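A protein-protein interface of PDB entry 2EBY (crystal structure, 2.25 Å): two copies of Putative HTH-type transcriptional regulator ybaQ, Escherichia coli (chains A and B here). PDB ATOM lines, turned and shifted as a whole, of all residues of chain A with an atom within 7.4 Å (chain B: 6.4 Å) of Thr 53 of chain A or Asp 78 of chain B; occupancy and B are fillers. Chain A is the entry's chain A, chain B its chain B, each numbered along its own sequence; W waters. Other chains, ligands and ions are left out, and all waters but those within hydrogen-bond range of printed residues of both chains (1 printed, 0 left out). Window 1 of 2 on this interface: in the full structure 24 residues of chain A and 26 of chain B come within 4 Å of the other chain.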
ATOM      1  N   ARG A  49       0.253  16.829  -3.555  1.00  0.00           N
ATOM      2  CA  ARG A  49      -0.804  17.460  -2.783  1.00  0.00           C
ATOM      3  C   ARG A  49      -0.260  17.554  -1.363  1.00  0.00           C
ATOM      4  O   ARG A  49       0.222  16.566  -0.812  1.00  0.00           O
ATOM      5  CB  ARG A  49      -2.051  16.570  -2.797  1.00  0.00           C
ATOM      6  CG  ARG A  49      -3.307  17.171  -2.183  1.00  0.00           C
ATOM      7  CD  ARG A  49      -4.191  16.071  -1.577  1.00  0.00           C
ATOM      8  NE  ARG A  49      -3.679  15.643  -0.272  1.00  0.00           N
ATOM      9  CZ  ARG A  49      -4.392  15.652   0.855  1.00  0.00           C
ATOM     10  NH1 ARG A  49      -5.658  16.054   0.844  1.00  0.00           N
ATOM     11  NH2 ARG A  49      -3.828  15.293   1.996  1.00  0.00           N
ATOM     12  N   LYS A  50      -0.329  18.732  -0.767  1.00  0.00           N
ATOM     13  CA  LYS A  50       0.163  18.885   0.591  1.00  0.00           C
ATOM     14  C   LYS A  50      -0.782  18.112   1.507  1.00  0.00           C
ATOM     15  O   LYS A  50      -1.955  17.935   1.183  1.00  0.00           O
ATOM     16  CB  LYS A  50       0.149  20.361   0.991  1.00  0.00           C
ATOM     17  CG  LYS A  50      -1.257  20.881   1.272  1.00  0.00           C
ATOM     18  CD  LYS A  50      -1.263  22.338   1.712  1.00  0.00           C
ATOM     19  CE  LYS A  50      -2.676  22.760   2.108  1.00  0.00           C
ATOM     20  NZ  LYS A  50      -2.765  24.176   2.568  1.00  0.00           N
ATOM     21  N   LEU A  51      -0.278  17.639   2.638  1.00  0.00           N
ATOM     22  CA  LEU A  51      -1.129  16.940   3.595  1.00  0.00           C
ATOM     23  C   LEU A  51      -1.997  18.033   4.222  1.00  0.00           C
ATOM     24  O   LEU A  51      -1.470  18.920   4.898  1.00  0.00           O
ATOM     25  CB  LEU A  51      -0.288  16.293   4.691  1.00  0.00           C
ATOM     26  CG  LEU A  51      -1.029  15.555   5.807  1.00  0.00           C
ATOM     27  CD1 LEU A  51      -1.272  14.112   5.406  1.00  0.00           C
ATOM     28  CD2 LEU A  51      -0.189  15.600   7.074  1.00  0.00           C
ATOM     29  N   THR A  52      -3.309  17.978   3.997  1.00  0.00           N
ATOM     30  CA  THR A  52      -4.214  18.986   4.552  1.00  0.00           C
ATOM     31  C   THR A  52      -4.588  18.645   5.994  1.00  0.00           C
ATOM     32  O   THR A  52      -4.343  17.526   6.462  1.00  0.00           O
ATOM     33  CB  THR A  52      -5.527  19.091   3.738  1.00  0.00           C
ATOM     34  OG1 THR A  52      -6.256  17.867   3.849  1.00  0.00           O
ATOM     35  CG2 THR A  52      -5.238  19.363   2.265  1.00  0.00           C
ATOM     36  N   THR A  53      -5.186  19.608   6.690  1.00  0.00           N
ATOM     37  CA  THR A  53      -5.612  19.412   8.073  1.00  0.00           C
ATOM     38  C   THR A  53      -6.638  18.279   8.151  1.00  0.00           C
ATOM     39  O   THR A  53      -6.542  17.398   9.010  1.00  0.00           O
ATOM     40  CB  THR A  53      -6.242  20.700   8.659  1.00  0.00           C
ATOM     41  OG1 THR A  53      -5.339  21.798   8.484  1.00  0.00           O
ATOM     42  CG2 THR A  53      -6.483  20.546  10.151  1.00  0.00           C
ATOM     43  N   GLU A  54      -7.617  18.306   7.253  1.00  0.00           N
ATOM     44  CA  GLU A  54      -8.648  17.270   7.230  1.00  0.00           C
ATOM     45  C   GLU A  54      -8.038  15.893   6.987  1.00  0.00           C
ATOM     46  O   GLU A  54      -8.379  14.932   7.677  1.00  0.00           O
ATOM     47  CB  GLU A  54      -9.698  17.554   6.146  1.00  0.00           C
ATOM     48  CG  GLU A  54     -10.885  16.591   6.181  1.00  0.00           C
ATOM     49  CD  GLU A  54     -11.924  16.873   5.102  1.00  0.00           C
ATOM     50  OE1 GLU A  54     -12.247  18.057   4.882  1.00  0.00           O
ATOM     51  OE2 GLU A  54     -12.432  15.911   4.484  1.00  0.00           O
ATOM     52  N   MET A  55      -7.140  15.785   6.012  1.00  0.00           N
ATOM     53  CA  MET A  55      -6.521  14.490   5.752  1.00  0.00           C
ATOM     54  C   MET A  55      -5.773  14.017   6.987  1.00  0.00           C
ATOM     55  O   MET A  55      -5.727  12.824   7.259  1.00  0.00           O
ATOM     56  CB  MET A  55      -5.545  14.547   4.572  1.00  0.00           C
ATOM     57  CG  MET A  55      -4.798  13.219   4.306  1.00  0.00           C
ATOM     58  SD  MET A  55      -5.831  11.798   3.792  1.00  0.00           S
ATOM     59  CE  MET A  55      -6.109  12.251   2.086  1.00  0.00           C
ATOM     60  N   ALA A  56      -5.177  14.957   7.716  1.00  0.00           N
ATOM     61  CA  ALA A  56      -4.428  14.631   8.930  1.00  0.00           C
ATOM     62  C   ALA A  56      -5.363  14.006   9.958  1.00  0.00           C
ATOM     63  O   ALA A  56      -4.984  13.072  10.651  1.00  0.00           O
ATOM     64  CB  ALA A  56      -3.774  15.887   9.507  1.00  0.00           C
ATOM     65  N   PHE A  57      -6.582  14.531  10.052  1.00  0.00           N
ATOM     66  CA  PHE A  57      -7.584  13.980  10.973  1.00  0.00           C
ATOM     67  C   PHE A  57      -7.939  12.543  10.577  1.00  0.00           C
ATOM     68  O   PHE A  57      -8.104  11.678  11.435  1.00  0.00           O
ATOM     69  CB  PHE A  57      -8.873  14.803  10.947  1.00  0.00           C
ATOM     70  CG  PHE A  57      -8.905  15.953  11.925  1.00  0.00           C
ATOM     71  CD1 PHE A  57      -8.067  17.053  11.768  1.00  0.00           C
ATOM     72  CD2 PHE A  57      -9.813  15.946  12.985  1.00  0.00           C
ATOM     73  CE1 PHE A  57      -8.136  18.131  12.646  1.00  0.00           C
ATOM     74  CE2 PHE A  57      -9.892  17.016  13.870  1.00  0.00           C
ATOM     75  CZ  PHE A  57      -9.052  18.116  13.704  1.00  0.00           C
ATOM     76  N   ARG A  58      -8.076  12.300   9.274  1.00  0.00           N
ATOM     77  CA  ARG A  58      -8.434  10.966   8.783  1.00  0.00           C
ATOM     78  C   ARG A  58      -7.325   9.961   9.079  1.00  0.00           C
ATOM     79  O   ARG A  58      -7.586   8.849   9.533  1.00  0.00           O
ATOM     80  CB  ARG A  58      -8.709  11.006   7.278  1.00  0.00           C
ATOM     81  CG  ARG A  58      -9.957  11.779   6.868  1.00  0.00           C
ATOM     82  CD  ARG A  58      -9.975  11.936   5.361  1.00  0.00           C
ATOM     83  NE  ARG A  58     -11.070  12.770   4.888  1.00  0.00           N
ATOM     84  CZ  ARG A  58     -12.331  12.367   4.793  1.00  0.00           C
ATOM     85  NH1 ARG A  58     -12.660  11.132   5.140  1.00  0.00           N
ATOM     86  NH2 ARG A  58     -13.263  13.198   4.347  1.00  0.00           N
ATOM     87  N   LEU A  59      -6.086  10.367   8.824  1.00  0.00           N
ATOM     88  CA  LEU A  59      -4.942   9.513   9.074  1.00  0.00           C
ATOM     89  C   LEU A  59      -4.803   9.230  10.573  1.00  0.00           C
ATOM     90  O   LEU A  59      -4.525   8.101  10.977  1.00  0.00           O
ATOM     91  CB  LEU A  59      -3.679  10.182   8.531  1.00  0.00           C
ATOM     92  CG  LEU A  59      -3.599  10.291   7.007  1.00  0.00           C
ATOM     93  CD1 LEU A  59      -2.430  11.186   6.610  1.00  0.00           C
ATOM     94  CD2 LEU A  59      -3.450   8.891   6.407  1.00  0.00           C
ATOM     95  N   VAL A  67      -3.161  14.229  15.458  1.00  0.00           N
ATOM     96  CA  VAL A  67      -3.275  14.924  14.189  1.00  0.00           C
ATOM     97  C   VAL A  67      -1.931  15.579  13.893  1.00  0.00           C
ATOM     98  O   VAL A  67      -1.468  15.601  12.755  1.00  0.00           O
ATOM     99  CB  VAL A  67      -4.352  16.027  14.234  1.00  0.00           C
ATOM    100  CG1 VAL A  67      -4.410  16.748  12.883  1.00  0.00           C
ATOM    101  CG2 VAL A  67      -5.711  15.421  14.576  1.00  0.00           C
ATOM    102  N   LEU A  71       0.715  16.468  10.801  1.00  0.00           N
ATOM    103  CA  LEU A  71       0.915  17.863  10.419  1.00  0.00           C
ATOM    104  C   LEU A  71       2.347  18.340  10.617  1.00  0.00           C
ATOM    105  O   LEU A  71       2.820  19.186   9.860  1.00  0.00           O
ATOM    106  CB  LEU A  71      -0.063  18.788  11.167  1.00  0.00           C
ATOM    107  CG  LEU A  71      -1.545  18.664  10.766  1.00  0.00           C
ATOM    108  CD1 LEU A  71      -2.385  19.649  11.594  1.00  0.00           C
ATOM    109  CD2 LEU A  71      -1.712  18.932   9.266  1.00  0.00           C
ATOM    110  N   LYS B  50      -5.360  31.835   4.085  1.00  0.00           N
ATOM    111  CA  LYS B  50      -4.562  31.238   5.143  1.00  0.00           C
ATOM    112  C   LYS B  50      -3.116  31.718   5.051  1.00  0.00           C
ATOM    113  O   LYS B  50      -2.617  32.021   3.971  1.00  0.00           O
ATOM    114  CB  LYS B  50      -4.600  29.712   5.049  1.00  0.00           C
ATOM    115  CG  LYS B  50      -5.940  29.114   5.439  1.00  0.00           C
ATOM    116  CD  LYS B  50      -5.869  27.600   5.490  1.00  0.00           C
ATOM    117  CE  LYS B  50      -7.209  27.009   5.916  1.00  0.00           C
ATOM    118  NZ  LYS B  50      -7.595  27.371   7.315  1.00  0.00           N
ATOM    119  N   LEU B  71       3.017  30.745  12.551  1.00  0.00           N
ATOM    120  CA  LEU B  71       2.478  29.461  12.115  1.00  0.00           C
ATOM    121  C   LEU B  71       1.552  28.809  13.142  1.00  0.00           C
ATOM    122  O   LEU B  71       0.559  28.184  12.774  1.00  0.00           O
ATOM    123  CB  LEU B  71       3.617  28.502  11.762  1.00  0.00           C
ATOM    124  CG  LEU B  71       4.447  28.872  10.525  1.00  0.00           C
ATOM    125  CD1 LEU B  71       5.575  27.856  10.321  1.00  0.00           C
ATOM    126  CD2 LEU B  71       3.528  28.912   9.311  1.00  0.00           C
ATOM    127  N   LEU B  73      -0.410  30.300  15.264  1.00  0.00           N
ATOM    128  CA  LEU B  73      -1.706  30.957  15.296  1.00  0.00           C
ATOM    129  C   LEU B  73      -2.542  30.348  14.162  1.00  0.00           C
ATOM    130  O   LEU B  73      -3.721  30.068  14.344  1.00  0.00           O
ATOM    131  CB  LEU B  73      -1.562  32.472  15.103  1.00  0.00           C
ATOM    132  CG  LEU B  73      -0.828  33.268  16.197  1.00  0.00           C
ATOM    133  CD1 LEU B  73      -0.531  34.662  15.708  1.00  0.00           C
ATOM    134  CD2 LEU B  73      -1.675  33.316  17.456  1.00  0.00           C
ATOM    135  N   GLN B  74      -1.932  30.126  13.000  1.00  0.00           N
ATOM    136  CA  GLN B  74      -2.671  29.551  11.869  1.00  0.00           C
ATOM    137  C   GLN B  74      -3.061  28.100  12.153  1.00  0.00           C
ATOM    138  O   GLN B  74      -4.168  27.680  11.830  1.00  0.00           O
ATOM    139  CB  GLN B  74      -1.844  29.616  10.573  1.00  0.00           C
ATOM    140  CG  GLN B  74      -2.612  29.154   9.330  1.00  0.00           C
ATOM    141  CD  GLN B  74      -3.832  30.017   9.034  1.00  0.00           C
ATOM    142  OE1 GLN B  74      -3.710  31.215   8.783  1.00  0.00           O
ATOM    143  NE2 GLN B  74      -5.019  29.406   9.065  1.00  0.00           N
ATOM    144  N   ALA B  75      -2.148  27.342  12.764  1.00  0.00           N
ATOM    145  CA  ALA B  75      -2.408  25.941  13.102  1.00  0.00           C
ATOM    146  C   ALA B  75      -3.629  25.797  14.002  1.00  0.00           C
ATOM    147  O   ALA B  75      -4.446  24.900  13.803  1.00  0.00           O
ATOM    148  CB  ALA B  75      -1.176  25.310  13.794  1.00  0.00           C
ATOM    149  N   ALA B  76      -3.755  26.665  15.001  1.00  0.00           N
ATOM    150  CA  ALA B  76      -4.889  26.573  15.913  1.00  0.00           C
ATOM    151  C   ALA B  76      -6.200  26.861  15.185  1.00  0.00           C
ATOM    152  O   ALA B  76      -7.214  26.221  15.439  1.00  0.00           O
ATOM    153  CB  ALA B  76      -4.704  27.532  17.096  1.00  0.00           C
ATOM    154  N   VAL B  77      -6.183  27.832  14.281  1.00  0.00           N
ATOM    155  CA  VAL B  77      -7.378  28.156  13.516  1.00  0.00           C
ATOM    156  C   VAL B  77      -7.755  26.969  12.620  1.00  0.00           C
ATOM    157  O   VAL B  77      -8.924  26.579  12.567  1.00  0.00           O
ATOM    158  CB  VAL B  77      -7.144  29.412  12.646  1.00  0.00           C
ATOM    159  CG1 VAL B  77      -8.269  29.583  11.636  1.00  0.00           C
ATOM    160  CG2 VAL B  77      -7.041  30.631  13.543  1.00  0.00           C
ATOM    161  N   ASP B  78      -6.769  26.404  11.922  1.00  0.00           N
ATOM    162  CA  ASP B  78      -7.011  25.257  11.035  1.00  0.00           C
ATOM    163  C   ASP B  78      -7.713  24.094  11.768  1.00  0.00           C
ATOM    164  O   ASP B  78      -8.676  23.521  11.252  1.00  0.00           O
ATOM    165  CB  ASP B  78      -5.697  24.719  10.432  1.00  0.00           C
ATOM    166  CG  ASP B  78      -5.042  25.680   9.439  1.00  0.00           C
ATOM    167  OD1 ASP B  78      -5.702  26.613   8.941  1.00  0.00           O
ATOM    168  OD2 ASP B  78      -3.851  25.486   9.139  1.00  0.00           O
ATOM    169  N   LEU B  79      -7.216  23.738  12.954  1.00  0.00           N
ATOM    170  CA  LEU B  79      -7.813  22.642  13.712  1.00  0.00           C
ATOM    171  C   LEU B  79      -9.232  23.023  14.108  1.00  0.00           C
ATOM    172  O   LEU B  79     -10.141  22.204  14.032  1.00  0.00           O
ATOM    173  CB  LEU B  79      -6.992  22.316  14.961  1.00  0.00           C
ATOM    174  CG  LEU B  79      -5.605  21.699  14.758  1.00  0.00           C
ATOM    175  CD1 LEU B  79      -4.934  21.509  16.123  1.00  0.00           C
ATOM    176  CD2 LEU B  79      -5.719  20.380  14.048  1.00  0.00           C
ATOM    177  N   TRP B  80      -9.409  24.277  14.518  1.00  0.00           N
ATOM    178  CA  TRP B  80     -10.714  24.770  14.911  1.00  0.00           C
ATOM    179  C   TRP B  80     -11.708  24.614  13.759  1.00  0.00           C
ATOM    180  O   TRP B  80     -12.843  24.194  13.974  1.00  0.00           O
ATOM    181  CB  TRP B  80     -10.632  26.244  15.305  1.00  0.00           C
ATOM    182  CG  TRP B  80     -11.929  26.810  15.756  1.00  0.00           C
ATOM    183  CD1 TRP B  80     -12.431  26.798  17.025  1.00  0.00           C
ATOM    184  CD2 TRP B  80     -12.905  27.458  14.940  1.00  0.00           C
ATOM    185  NE1 TRP B  80     -13.661  27.404  17.053  1.00  0.00           N
ATOM    186  CE2 TRP B  80     -13.978  27.822  15.788  1.00  0.00           C
ATOM    187  CE3 TRP B  80     -12.982  27.771  13.578  1.00  0.00           C
ATOM    188  CZ2 TRP B  80     -15.118  28.481  15.314  1.00  0.00           C
ATOM    189  CZ3 TRP B  80     -14.112  28.425  13.103  1.00  0.00           C
ATOM    190  CH2 TRP B  80     -15.166  28.777  13.973  1.00  0.00           C
ATOM    191  N   GLU B  81     -11.286  24.949  12.539  1.00  0.00           N
ATOM    192  CA  GLU B  81     -12.181  24.844  11.391  1.00  0.00           C
ATOM    193  C   GLU B  81     -12.637  23.410  11.144  1.00  0.00           C
ATOM    194  O   GLU B  81     -13.805  23.179  10.851  1.00  0.00           O
ATOM    195  CB  GLU B  81     -11.530  25.419  10.129  1.00  0.00           C
ATOM    196  CG  GLU B  81     -11.150  26.888  10.263  1.00  0.00           C
ATOM    197  CD  GLU B  81     -10.614  27.479   8.975  1.00  0.00           C
ATOM    198  OE1 GLU B  81      -9.908  26.755   8.248  1.00  0.00           O
ATOM    199  OE2 GLU B  81     -10.882  28.671   8.694  1.00  0.00           O
ATOM    200  N   VAL B  82     -11.731  22.445  11.265  1.00  0.00           N
ATOM    201  CA  VAL B  82     -12.115  21.053  11.051  1.00  0.00           C
ATOM    202  C   VAL B  82     -12.980  20.522  12.198  1.00  0.00           C
ATOM    203  O   VAL B  82     -13.907  19.747  11.957  1.00  0.00           O
ATOM    204  CB  VAL B  82     -10.881  20.129  10.864  1.00  0.00           C
ATOM    205  CG1 VAL B  82     -11.322  18.682  10.751  1.00  0.00           C
ATOM    206  CG2 VAL B  82     -10.131  20.525   9.600  1.00  0.00           C
ATOM    207  N   GLU B  83     -12.691  20.936  13.434  1.00  0.00           N
ATOM    208  CA  GLU B  83     -13.481  20.483  14.575  1.00  0.00           C
ATOM    209  C   GLU B  83     -14.915  20.986  14.459  1.00  0.00           C
ATOM    210  O   GLU B  83     -15.847  20.323  14.898  1.00  0.00           O
ATOM    211  CB  GLU B  83     -12.879  20.986  15.900  1.00  0.00           C
ATOM    212  CG  GLU B  83     -11.517  20.407  16.241  1.00  0.00           C
ATOM    213  CD  GLU B  83     -11.567  18.959  16.713  1.00  0.00           C
ATOM    214  OE1 GLU B  83     -12.637  18.320  16.614  1.00  0.00           O
ATOM    215  OE2 GLU B  83     -10.520  18.461  17.186  1.00  0.00           O
HETATM  216  O   HOH W   1      -2.930  23.073   9.455  1.00  0.00           O
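2 positions are printed for both chains.
Water W1 lies within hydrogen-bond range of the side-chain carboxylate (OD2) of Asp 78 of chain B (2.6 Å) and the side-chain hydroxyl (OG1) of Thr 53 of chain A (2.9 Å).
Thr 53 of chain A touches just these residues of chain B: Asp 78 (3.5 Å), Leu 79 (3.97 Å) and Val 82 (3.7 Å). Of the printed residues of chain A, Asp 78 of chain B touches Thr 53 (3.5 Å). Of the printed residues of chain A, Leu 79 of chain B touches Thr 53 (3.97 Å) and Phe 57 (3.6 Å). Of the printed residues of chain A, Glu 83 of chain B touches Phe 57. Of the printed residues of chain A, Val 82 of chain B touches Thr 53 and Phe 57. Of the printed residues of chain B, Phe 57 of chain A touches Leu 79 (3.6 Å), Val 82 (3.7 Å) and Glu 83 (3.7 Å). Arg 58 of chain A touches none of the printed residues of chain B. The nearest printed residue of chain A that does not touch Glu 83 of chain B is Val 67 of chain A (6.3 Å).
NZ of Lys 50 of chain B is in salt-bridge range of OD1 of Asp 78 of chain B, 2.6 Å away. NE2 of Gln 74 of chain B lies within hydrogen-bond range of OD1 of Asp 78 of chain B, 2.9 Å away.
Printed residues of chain A that touch a printed residue of chain B: Thr 53 and Phe 57. Hydrophobic or aromatic side chains of chain A within 4 Å of the printed part of chain B: Phe 57. Hydrophobic or aromatic side chains of chain B within 4 Å of the printed part of chain A: Leu 79 and Val 82. Among the printed residues, 6 pairs touch across the chains.
OG1 of Thr 53 of chain A touches CB of Asp 78 of chain B, at 3.5 Å. Thr 53 of chain A touches Leu 79 of chain B (CG2 to CD2, 3.97 Å). Val 82 of chain B touches Thr 53 of chain A (CG2 to CG2, 3.7 Å). Phe 57 of chain A touches Leu 79 of chain B. Phe 57 of chain A touches Val 82 of chain B (CE1 to CG1, 3.7 Å). Glu 83 of chain B touches Phe 57 of chain A.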
